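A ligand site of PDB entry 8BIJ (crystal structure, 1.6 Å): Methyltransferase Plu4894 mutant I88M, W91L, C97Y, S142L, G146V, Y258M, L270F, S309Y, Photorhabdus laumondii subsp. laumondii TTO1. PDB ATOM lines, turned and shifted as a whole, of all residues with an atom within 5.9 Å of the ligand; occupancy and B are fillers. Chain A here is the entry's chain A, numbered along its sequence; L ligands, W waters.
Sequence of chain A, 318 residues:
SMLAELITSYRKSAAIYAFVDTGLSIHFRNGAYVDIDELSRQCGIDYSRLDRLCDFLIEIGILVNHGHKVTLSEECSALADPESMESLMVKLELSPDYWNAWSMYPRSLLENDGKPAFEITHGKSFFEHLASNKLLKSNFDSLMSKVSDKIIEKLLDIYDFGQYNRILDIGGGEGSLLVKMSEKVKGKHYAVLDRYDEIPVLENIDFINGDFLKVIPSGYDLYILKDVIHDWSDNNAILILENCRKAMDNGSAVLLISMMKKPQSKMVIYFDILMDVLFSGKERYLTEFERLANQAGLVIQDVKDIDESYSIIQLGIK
The guanidinium group (NE) of Arg 195 lies close to a nitrogen (N4) of the ligand.
O of Asp 227 sits close to S1 of the ligand, at 3.7 Å.
Residues that only touch the ligand: Asp 231 (3.3 Å), Met 144 (3.4 Å), Phe 127 (3.6 Å), Trp 232 (3.6 Å), Gly 173 (3.7 Å), Phe 140 (3.8 Å), Gly 172 (3.9 Å), Leu 213 (3.9 Å), Gly 210 (3.9 Å), Ser 148 (3.9 Å) and Leu 193 (3.995 Å).
Hydrophobic or aromatic side chains within 4 Å of the ligand: Phe 127, Phe 140, Met 144, Leu 193, Phe 212, Leu 213 and Trp 232.
Within 4 Å of the ligand: Phe 127, Phe 140, Met 144, Ser 148, Gly 171, Gly 172, Gly 173, Leu 193, Asp 194, Arg 195, Gly 210, Asp 211, Phe 212, Leu 213, Lys 226, Asp 227, Asp 231 and Trp 232.
The nearest printed residue that does not touch the ligand is Val 228 (4.3 Å).
N5 of the ligand is in hydrogen-bond range of N of Phe 212 (3.1 Å).
The backbone carbonyl oxygen of Lys 226 is in hydrogen-bond range of a nitrogen (N1) of the ligand (2.8 Å).
O of Gly 171 sits at hydrogen-bond distance from N1 of the ligand (2.8 Å).
The side-chain carboxylate of Asp 211 is in hydrogen-bond range of a nitrogen (N4) of the ligand (2.8 Å).
An oxygen (O2) of the ligand is in salt-bridge range of the side-chain amino group (NZ) of Lys 226 (2.7 Å).
O5 of the ligand is in hydrogen-bond range of OD1 of Asp 194 (2.6 Å).
The backbone carbonyl oxygen (O) of Leu 193 sits at hydrogen-bond distance from the backbone NH (N) of Gly 172 (3.3 Å).
The side-chain carboxylate (OD2) of Asp 211 lies within salt-bridge range of the guanidinium group (NH2) of Arg 195 (3.1 Å).
The indole nitrogen (NE1) of Trp 232 lies close to the backbone carbonyl oxygen (O) of Val 228.
O of Met 144 is in hydrogen-bond range of OG of Ser 148.
O of Asp 169 lies within hydrogen-bond range of N of Leu 193.
The side-chain amino group (NZ) of Lys 226 lies within salt-bridge range of the side-chain carboxylate (OD2) of Asp 227 (3.0 Å).
The backbone NH of Gly 171 lies within hydrogen-bond range of the backbone carbonyl oxygen of Leu 193 (2.6 Å).
The side-chain carboxylate of Asp 211 sits at hydrogen-bond distance from the backbone NH of Leu 213 (3.0 Å).
Water W5 lies within hydrogen-bond range of OD2 of Asp 169 and N1 of the ligand.
Water W6 lies within hydrogen-bond range of OD1 of Asp 169, O of Ile 170, N of Lys 226 and N1 of the ligand.
Water W3 lies within hydrogen-bond range of OD2 of Asp 231 (2.8 Å), O3 of the ligand (3.0 Å) and NE1 of Trp 232 (3.0 Å).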
ATOM      1  N   PHE A 127      35.282   9.960  32.252  1.00  0.00           N
ATOM      2  CA  PHE A 127      34.374   9.345  31.248  1.00  0.00           C
ATOM      3  C   PHE A 127      34.941   8.018  30.723  1.00  0.00           C
ATOM      4  O   PHE A 127      34.133   7.105  30.471  1.00  0.00           O
ATOM      5  CB  PHE A 127      33.969  10.326  30.143  1.00  0.00           C
ATOM      6  CG  PHE A 127      33.071  11.426  30.675  1.00  0.00           C
ATOM      7  CD1 PHE A 127      31.877  11.095  31.316  1.00  0.00           C
ATOM      8  CD2 PHE A 127      33.431  12.760  30.589  1.00  0.00           C
ATOM      9  CE1 PHE A 127      31.071  12.083  31.862  1.00  0.00           C
ATOM     10  CE2 PHE A 127      32.613  13.743  31.129  1.00  0.00           C
ATOM     11  CZ  PHE A 127      31.442  13.404  31.766  1.00  0.00           C
ATOM     12  N   LYS A 137      28.829   3.574  34.707  1.00  0.00           N
ATOM     13  CA  LYS A 137      28.173   4.404  33.671  1.00  0.00           C
ATOM     14  C   LYS A 137      26.697   4.601  34.023  1.00  0.00           C
ATOM     15  O   LYS A 137      26.208   5.736  33.893  1.00  0.00           O
ATOM     16  CB  LYS A 137      28.309   3.775  32.278  1.00  0.00           C
ATOM     17  CG  LYS A 137      27.881   4.672  31.124  1.00  0.00           C
ATOM     18  CD  LYS A 137      28.411   4.229  29.771  1.00  0.00           C
ATOM     19  CE  LYS A 137      29.103   5.350  29.009  1.00  0.00           C
ATOM     20  NZ  LYS A 137      29.779   4.847  27.780  1.00  0.00           N
ATOM     21  N   PHE A 140      25.816   6.825  37.478  1.00  0.00           N
ATOM     22  CA  PHE A 140      25.949   8.249  37.074  1.00  0.00           C
ATOM     23  C   PHE A 140      24.683   8.667  36.316  1.00  0.00           C
ATOM     24  O   PHE A 140      24.221   9.808  36.519  1.00  0.00           O
ATOM     25  CB  PHE A 140      27.222   8.414  36.241  1.00  0.00           C
ATOM     26  CG  PHE A 140      27.484   9.815  35.762  1.00  0.00           C
ATOM     27  CD1 PHE A 140      27.986  10.775  36.626  1.00  0.00           C
ATOM     28  CD2 PHE A 140      27.210  10.173  34.458  1.00  0.00           C
ATOM     29  CE1 PHE A 140      28.217  12.065  36.192  1.00  0.00           C
ATOM     30  CE2 PHE A 140      27.448  11.470  34.021  1.00  0.00           C
ATOM     31  CZ  PHE A 140      27.959  12.408  34.888  1.00  0.00           C
ATOM     32  N   MET A 144      22.134  11.767  37.008  1.00  0.00           N
ATOM     33  CA  MET A 144      21.893  12.788  35.964  1.00  0.00           C
ATOM     34  C   MET A 144      20.387  12.868  35.662  1.00  0.00           C
ATOM     35  O   MET A 144      19.861  13.989  35.553  1.00  0.00           O
ATOM     36  CB  MET A 144      22.674  12.491  34.675  1.00  0.00           C
ATOM     37  CG  MET A 144      24.178  12.654  34.788  1.00  0.00           C
ATOM     38  SD  MET A 144      24.751  14.311  35.259  1.00  0.00           S
ATOM     39  CE  MET A 144      24.779  14.207  37.046  1.00  0.00           C
ATOM     40  N   SER A 145      19.721  11.710  35.570  1.00  0.00           N
ATOM     41  CA  SER A 145      18.262  11.581  35.291  1.00  0.00           C
ATOM     42  C   SER A 145      17.445  12.291  36.375  1.00  0.00           C
ATOM     43  O   SER A 145      16.467  12.968  36.017  1.00  0.00           O
ATOM     44  CB  SER A 145      17.860  10.140  35.153  1.00  0.00           C
ATOM     45  OG  SER A 145      18.650   9.491  34.158  1.00  0.00           O
ATOM     46  N   SER A 148      17.917  16.078  35.989  1.00  0.00           N
ATOM     47  CA  SER A 148      17.068  16.498  34.835  1.00  0.00           C
ATOM     48  C   SER A 148      15.612  16.592  35.298  1.00  0.00           C
ATOM     49  O   SER A 148      14.990  17.644  35.079  1.00  0.00           O
ATOM     50  CB  SER A 148      17.236  15.591  33.653  1.00  0.00           C
ATOM     51  OG  SER A 148      18.445  15.877  32.969  1.00  0.00           O
ATOM     52  N   ASP A 169      20.374  17.463  21.856  1.00  0.00           N
ATOM     53  CA  ASP A 169      20.978  17.530  23.218  1.00  0.00           C
ATOM     54  C   ASP A 169      22.409  16.986  23.112  1.00  0.00           C
ATOM     55  O   ASP A 169      22.551  15.753  22.960  1.00  0.00           O
ATOM     56  CB  ASP A 169      20.105  16.794  24.221  1.00  0.00           C
ATOM     57  CG  ASP A 169      20.510  17.041  25.662  1.00  0.00           C
ATOM     58  OD1 ASP A 169      21.442  17.847  25.873  1.00  0.00           O
ATOM     59  OD2 ASP A 169      19.867  16.471  26.553  1.00  0.00           O
ATOM     60  N   ILE A 170      23.399  17.878  23.136  1.00  0.00           N
ATOM     61  CA  ILE A 170      24.848  17.544  22.954  1.00  0.00           C
ATOM     62  C   ILE A 170      25.378  17.041  24.293  1.00  0.00           C
ATOM     63  O   ILE A 170      25.305  17.812  25.255  1.00  0.00           O
ATOM     64  CB  ILE A 170      25.650  18.756  22.430  1.00  0.00           C
ATOM     65  CG1 ILE A 170      25.089  19.315  21.122  1.00  0.00           C
ATOM     66  CG2 ILE A 170      27.112  18.394  22.281  1.00  0.00           C
ATOM     67  CD1 ILE A 170      25.632  20.682  20.794  1.00  0.00           C
ATOM     68  N   GLY A 171      25.878  15.803  24.334  1.00  0.00           N
ATOM     69  CA  GLY A 171      26.278  15.130  25.589  1.00  0.00           C
ATOM     70  C   GLY A 171      25.065  14.882  26.463  1.00  0.00           C
ATOM     71  O   GLY A 171      25.154  15.070  27.684  1.00  0.00           O
ATOM     72  N   GLY A 172      23.936  14.496  25.862  1.00  0.00           N
ATOM     73  CA  GLY A 172      22.660  14.305  26.583  1.00  0.00           C
ATOM     74  C   GLY A 172      22.552  12.954  27.264  1.00  0.00           C
ATOM     75  O   GLY A 172      21.505  12.696  27.899  1.00  0.00           O
ATOM     76  N   GLY A 173      23.562  12.089  27.118  1.00  0.00           N
ATOM     77  CA  GLY A 173      23.632  10.795  27.829  1.00  0.00           C
ATOM     78  C   GLY A 173      22.442   9.915  27.502  1.00  0.00           C
ATOM     79  O   GLY A 173      22.223   9.658  26.302  1.00  0.00           O
ATOM     80  N   GLU A 174      21.676   9.497  28.515  1.00  0.00           N
ATOM     81  CA  GLU A 174      20.509   8.576  28.357  1.00  0.00           C
ATOM     82  C   GLU A 174      19.277   9.329  27.838  1.00  0.00           C
ATOM     83  O   GLU A 174      18.264   8.665  27.539  1.00  0.00           O
ATOM     84  CB  GLU A 174      20.227   7.846  29.671  1.00  0.00           C
ATOM     85  CG  GLU A 174      21.254   6.770  29.976  1.00  0.00           C
ATOM     86  CD  GLU A 174      21.403   5.716  28.884  1.00  0.00           C
ATOM     87  OE1 GLU A 174      20.405   5.028  28.594  1.00  0.00           O
ATOM     88  OE2 GLU A 174      22.499   5.617  28.301  1.00  0.00           O
ATOM     89  N   SER A 176      17.346  11.778  29.242  1.00  0.00           N
ATOM     90  CA  SER A 176      16.242  12.015  30.219  1.00  0.00           C
ATOM     91  C   SER A 176      15.667  13.430  30.045  1.00  0.00           C
ATOM     92  O   SER A 176      14.438  13.574  30.206  1.00  0.00           O
ATOM     93  CB  SER A 176      16.688  11.752  31.637  1.00  0.00           C
ATOM     94  OG  SER A 176      17.896  12.437  31.913  1.00  0.00           O
ATOM     95  N   LEU A 193      23.203  13.383  21.255  1.00  0.00           N
ATOM     96  CA  LEU A 193      24.575  13.002  20.847  1.00  0.00           C
ATOM     97  C   LEU A 193      25.387  12.714  22.100  1.00  0.00           C
ATOM     98  O   LEU A 193      25.388  13.566  23.007  1.00  0.00           O
ATOM     99  CB  LEU A 193      25.213  14.123  20.024  1.00  0.00           C
ATOM    100  CG  LEU A 193      26.561  13.754  19.405  1.00  0.00           C
ATOM    101  CD1 LEU A 193      26.764  14.432  18.058  1.00  0.00           C
ATOM    102  CD2 LEU A 193      27.705  14.084  20.335  1.00  0.00           C
ATOM    103  N   ASP A 194      26.047  11.563  22.130  1.00  0.00           N
ATOM    104  CA  ASP A 194      26.928  11.172  23.257  1.00  0.00           C
ATOM    105  C   ASP A 194      27.845  10.048  22.781  1.00  0.00           C
ATOM    106  O   ASP A 194      27.790   9.687  21.600  1.00  0.00           O
ATOM    107  CB  ASP A 194      26.088  10.795  24.481  1.00  0.00           C
ATOM    108  CG  ASP A 194      26.770  11.143  25.791  1.00  0.00           C
ATOM    109  OD1 ASP A 194      27.858  10.584  26.056  1.00  0.00           O
ATOM    110  OD2 ASP A 194      26.220  11.987  26.517  1.00  0.00           O
ATOM    111  N   ARG A 195      28.696   9.531  23.661  1.00  0.00           N
ATOM    112  CA  ARG A 195      29.558   8.354  23.389  1.00  0.00           C
ATOM    113  C   ARG A 195      28.839   7.116  23.939  1.00  0.00           C
ATOM    114  O   ARG A 195      28.739   6.997  25.168  1.00  0.00           O
ATOM    115  CB  ARG A 195      30.931   8.544  24.048  1.00  0.00           C
ATOM    116  CG  ARG A 195      31.779   9.649  23.437  1.00  0.00           C
ATOM    117  CD  ARG A 195      33.047   9.842  24.247  1.00  0.00           C
ATOM    118  NE  ARG A 195      34.196  10.309  23.482  1.00  0.00           N
ATOM    119  CZ  ARG A 195      35.173   9.541  22.993  1.00  0.00           C
ATOM    120  NH1 ARG A 195      35.161   8.234  23.153  1.00  0.00           N
ATOM    121  NH2 ARG A 195      36.166  10.110  22.324  1.00  0.00           N
ATOM    122  N   GLY A 210      28.546   9.729  18.833  1.00  0.00           N
ATOM    123  CA  GLY A 210      29.448  10.758  18.269  1.00  0.00           C
ATOM    124  C   GLY A 210      30.439  11.279  19.274  1.00  0.00           C
ATOM    125  O   GLY A 210      30.570  10.684  20.366  1.00  0.00           O
ATOM    126  N   ASP A 211      31.112  12.373  18.903  1.00  0.00           N
ATOM    127  CA  ASP A 211      32.209  12.985  19.704  1.00  0.00           C
ATOM    128  C   ASP A 211      32.175  14.493  19.471  1.00  0.00           C
ATOM    129  O   ASP A 211      32.604  14.941  18.377  1.00  0.00           O
ATOM    130  CB  ASP A 211      33.563  12.373  19.320  1.00  0.00           C
ATOM    131  CG  ASP A 211      34.734  12.866  20.146  1.00  0.00           C
ATOM    132  OD1 ASP A 211      34.555  13.870  20.862  1.00  0.00           O
ATOM    133  OD2 ASP A 211      35.810  12.228  20.077  1.00  0.00           O
ATOM    134  N   PHE A 212      31.652  15.250  20.438  1.00  0.00           N
ATOM    135  CA  PHE A 212      31.430  16.718  20.304  1.00  0.00           C
ATOM    136  C   PHE A 212      32.763  17.473  20.263  1.00  0.00           C
ATOM    137  O   PHE A 212      32.712  18.675  19.978  1.00  0.00           O
ATOM    138  CB  PHE A 212      30.476  17.265  21.371  1.00  0.00           C
ATOM    139  CG  PHE A 212      30.818  17.015  22.821  1.00  0.00           C
ATOM    140  CD1 PHE A 212      32.073  17.301  23.333  1.00  0.00           C
ATOM    141  CD2 PHE A 212      29.831  16.594  23.697  1.00  0.00           C
ATOM    142  CE1 PHE A 212      32.349  17.101  24.680  1.00  0.00           C
ATOM    143  CE2 PHE A 212      30.096  16.403  25.039  1.00  0.00           C
ATOM    144  CZ  PHE A 212      31.372  16.648  25.531  1.00  0.00           C
ATOM    145  N   LEU A 213      33.892  16.813  20.554  1.00  0.00           N
ATOM    146  CA  LEU A 213      35.244  17.412  20.384  1.00  0.00           C
ATOM    147  C   LEU A 213      35.653  17.380  18.904  1.00  0.00           C
ATOM    148  O   LEU A 213      36.560  18.150  18.535  1.00  0.00           O
ATOM    149  CB  LEU A 213      36.246  16.679  21.268  1.00  0.00           C
ATOM    150  CG  LEU A 213      35.974  16.751  22.778  1.00  0.00           C
ATOM    151  CD1 LEU A 213      36.974  15.890  23.553  1.00  0.00           C
ATOM    152  CD2 LEU A 213      36.006  18.184  23.269  1.00  0.00           C
ATOM    153  N   LEU A 225      23.384  22.296  25.544  1.00  0.00           N
ATOM    154  CA  LEU A 225      24.553  21.845  26.345  1.00  0.00           C
ATOM    155  C   LEU A 225      24.229  21.975  27.839  1.00  0.00           C
ATOM    156  O   LEU A 225      24.383  23.095  28.380  1.00  0.00           O
ATOM    157  CB  LEU A 225      25.770  22.684  25.949  1.00  0.00           C
ATOM    158  CG  LEU A 225      26.412  22.314  24.613  1.00  0.00           C
ATOM    159  CD1 LEU A 225      27.260  23.465  24.084  1.00  0.00           C
ATOM    160  CD2 LEU A 225      27.248  21.041  24.723  1.00  0.00           C
ATOM    161  N   LYS A 226      23.743  20.885  28.452  1.00  0.00           N
ATOM    162  CA  LYS A 226      23.376  20.862  29.893  1.00  0.00           C
ATOM    163  C   LYS A 226      24.479  20.149  30.670  1.00  0.00           C
ATOM    164  O   LYS A 226      24.735  18.964  30.408  1.00  0.00           O
ATOM    165  CB  LYS A 226      22.030  20.183  30.163  1.00  0.00           C
ATOM    166  CG  LYS A 226      21.663  20.118  31.644  1.00  0.00           C
ATOM    167  CD  LYS A 226      20.387  19.356  31.948  1.00  0.00           C
ATOM    168  CE  LYS A 226      20.201  19.117  33.423  1.00  0.00           C
ATOM    169  NZ  LYS A 226      21.215  18.180  33.970  1.00  0.00           N
ATOM    170  N   ASP A 227      25.110  20.866  31.595  1.00  0.00           N
ATOM    171  CA  ASP A 227      26.094  20.261  32.541  1.00  0.00           C
ATOM    172  C   ASP A 227      27.204  19.583  31.734  1.00  0.00           C
ATOM    173  O   ASP A 227      27.745  18.526  32.183  1.00  0.00           O
ATOM    174  CB  ASP A 227      25.376  19.320  33.512  1.00  0.00           C
ATOM    175  CG  ASP A 227      24.645  20.038  34.640  1.00  0.00           C
ATOM    176  OD1 ASP A 227      25.142  21.099  35.060  1.00  0.00           O
ATOM    177  OD2 ASP A 227      23.597  19.525  35.103  1.00  0.00           O
ATOM    178  N   VAL A 228      27.570  20.188  30.592  1.00  0.00           N
ATOM    179  CA  VAL A 228      28.689  19.734  29.718  1.00  0.00           C
ATOM    180  C   VAL A 228      29.876  20.681  29.881  1.00  0.00           C
ATOM    181  O   VAL A 228      30.974  20.187  30.188  1.00  0.00           O
ATOM    182  CB  VAL A 228      28.241  19.617  28.247  1.00  0.00           C
ATOM    183  CG1 VAL A 228      29.426  19.447  27.305  1.00  0.00           C
ATOM    184  CG2 VAL A 228      27.244  18.482  28.069  1.00  0.00           C
ATOM    185  N   ASP A 231      32.618  20.561  32.564  1.00  0.00           N
ATOM    186  CA  ASP A 231      33.512  19.373  32.594  1.00  0.00           C
ATOM    187  C   ASP A 231      34.856  19.679  31.925  1.00  0.00           C
ATOM    188  O   ASP A 231      35.723  18.779  31.923  1.00  0.00           O
ATOM    189  CB  ASP A 231      32.914  18.157  31.870  1.00  0.00           C
ATOM    190  CG  ASP A 231      31.657  17.586  32.478  1.00  0.00           C
ATOM    191  OD1 ASP A 231      31.361  17.919  33.647  1.00  0.00           O
ATOM    192  OD2 ASP A 231      30.976  16.820  31.779  1.00  0.00           O
ATOM    193  N   TRP A 232      35.049  20.878  31.352  1.00  0.00           N
ATOM    194  CA  TRP A 232      36.115  21.115  30.352  1.00  0.00           C
ATOM    195  C   TRP A 232      36.952  22.350  30.688  1.00  0.00           C
ATOM    196  O   TRP A 232      36.401  23.327  31.239  1.00  0.00           O
ATOM    197  CB  TRP A 232      35.517  21.205  28.935  1.00  0.00           C
ATOM    198  CG  TRP A 232      34.828  19.932  28.569  1.00  0.00           C
ATOM    199  CD1 TRP A 232      33.493  19.683  28.644  1.00  0.00           C
ATOM    200  CD2 TRP A 232      35.448  18.708  28.141  1.00  0.00           C
ATOM    201  NE1 TRP A 232      33.221  18.398  28.275  1.00  0.00           N
ATOM    202  CE2 TRP A 232      34.404  17.781  27.939  1.00  0.00           C
ATOM    203  CE3 TRP A 232      36.761  18.312  27.876  1.00  0.00           C
ATOM    204  CZ2 TRP A 232      34.644  16.472  27.506  1.00  0.00           C
ATOM    205  CZ3 TRP A 232      36.997  17.024  27.449  1.00  0.00           C
ATOM    206  CH2 TRP A 232      35.949  16.124  27.268  1.00  0.00           C
HETATM  207  N1  LIG L   1      23.688  16.572  29.523  1.00  0.00           N
HETATM  208  C1  LIG L   1      23.522  15.386  30.442  1.00  0.00           C
HETATM  209  C2  LIG L   1      24.850  14.735  30.836  1.00  0.00           C
HETATM  210  C3  LIG L   1      25.842  15.674  31.482  1.00  0.00           C
HETATM  211  S1  LIG L   1      27.391  14.837  31.974  1.00  0.00           S
HETATM  212  C4  LIG L   1      22.781  15.833  31.700  1.00  0.00           C
HETATM  213  O1  LIG L   1      22.245  14.977  32.417  1.00  0.00           O
HETATM  214  O2  LIG L   1      22.715  17.034  32.025  1.00  0.00           O
HETATM  215  C5  LIG L   1      28.430  15.072  30.510  1.00  0.00           C
HETATM  216  C6  LIG L   1      28.059  14.227  29.309  1.00  0.00           C
HETATM  217  O3  LIG L   1      29.023  14.467  28.254  1.00  0.00           O
HETATM  218  C7  LIG L   1      28.085  12.703  29.556  1.00  0.00           C
HETATM  219  O4  LIG L   1      26.856  12.109  29.168  1.00  0.00           O
HETATM  220  C8  LIG L   1      29.280  12.222  28.723  1.00  0.00           C
HETATM  221  O5  LIG L   1      29.158  10.892  28.275  1.00  0.00           O
HETATM  222  C9  LIG L   1      29.265  13.254  27.599  1.00  0.00           C
HETATM  223  N2  LIG L   1      30.515  13.350  26.862  1.00  0.00           N
HETATM  224  C10 LIG L   1      31.777  13.476  27.386  1.00  0.00           C
HETATM  225  N3  LIG L   1      32.709  13.576  26.479  1.00  0.00           N
HETATM  226  C11 LIG L   1      32.027  13.500  25.273  1.00  0.00           C
HETATM  227  C12 LIG L   1      32.456  13.547  23.929  1.00  0.00           C
HETATM  228  N4  LIG L   1      33.730  13.699  23.574  1.00  0.00           N
HETATM  229  N5  LIG L   1      31.507  13.462  22.963  1.00  0.00           N
HETATM  230  C13 LIG L   1      30.227  13.308  23.335  1.00  0.00           C
HETATM  231  N6  LIG L   1      29.699  13.266  24.562  1.00  0.00           N
HETATM  232  C14 LIG L   1      30.668  13.361  25.494  1.00  0.00           C
HETATM  233  O   HOH W   1      28.999  16.889  34.284  1.00  0.00           O
HETATM  234  O   HOH W   2      31.570   9.724  27.515  1.00  0.00           O
HETATM  235  O   HOH W   3      31.046  16.505  29.001  1.00  0.00           O
HETATM  236  O   HOH W   4      35.317  12.658  26.739  1.00  0.00           O
HETATM  237  O   HOH W   5      20.906  16.763  28.899  1.00  0.00           O
HETATM  238  O   HOH W   6      23.500  18.307  27.186  1.00  0.00           O
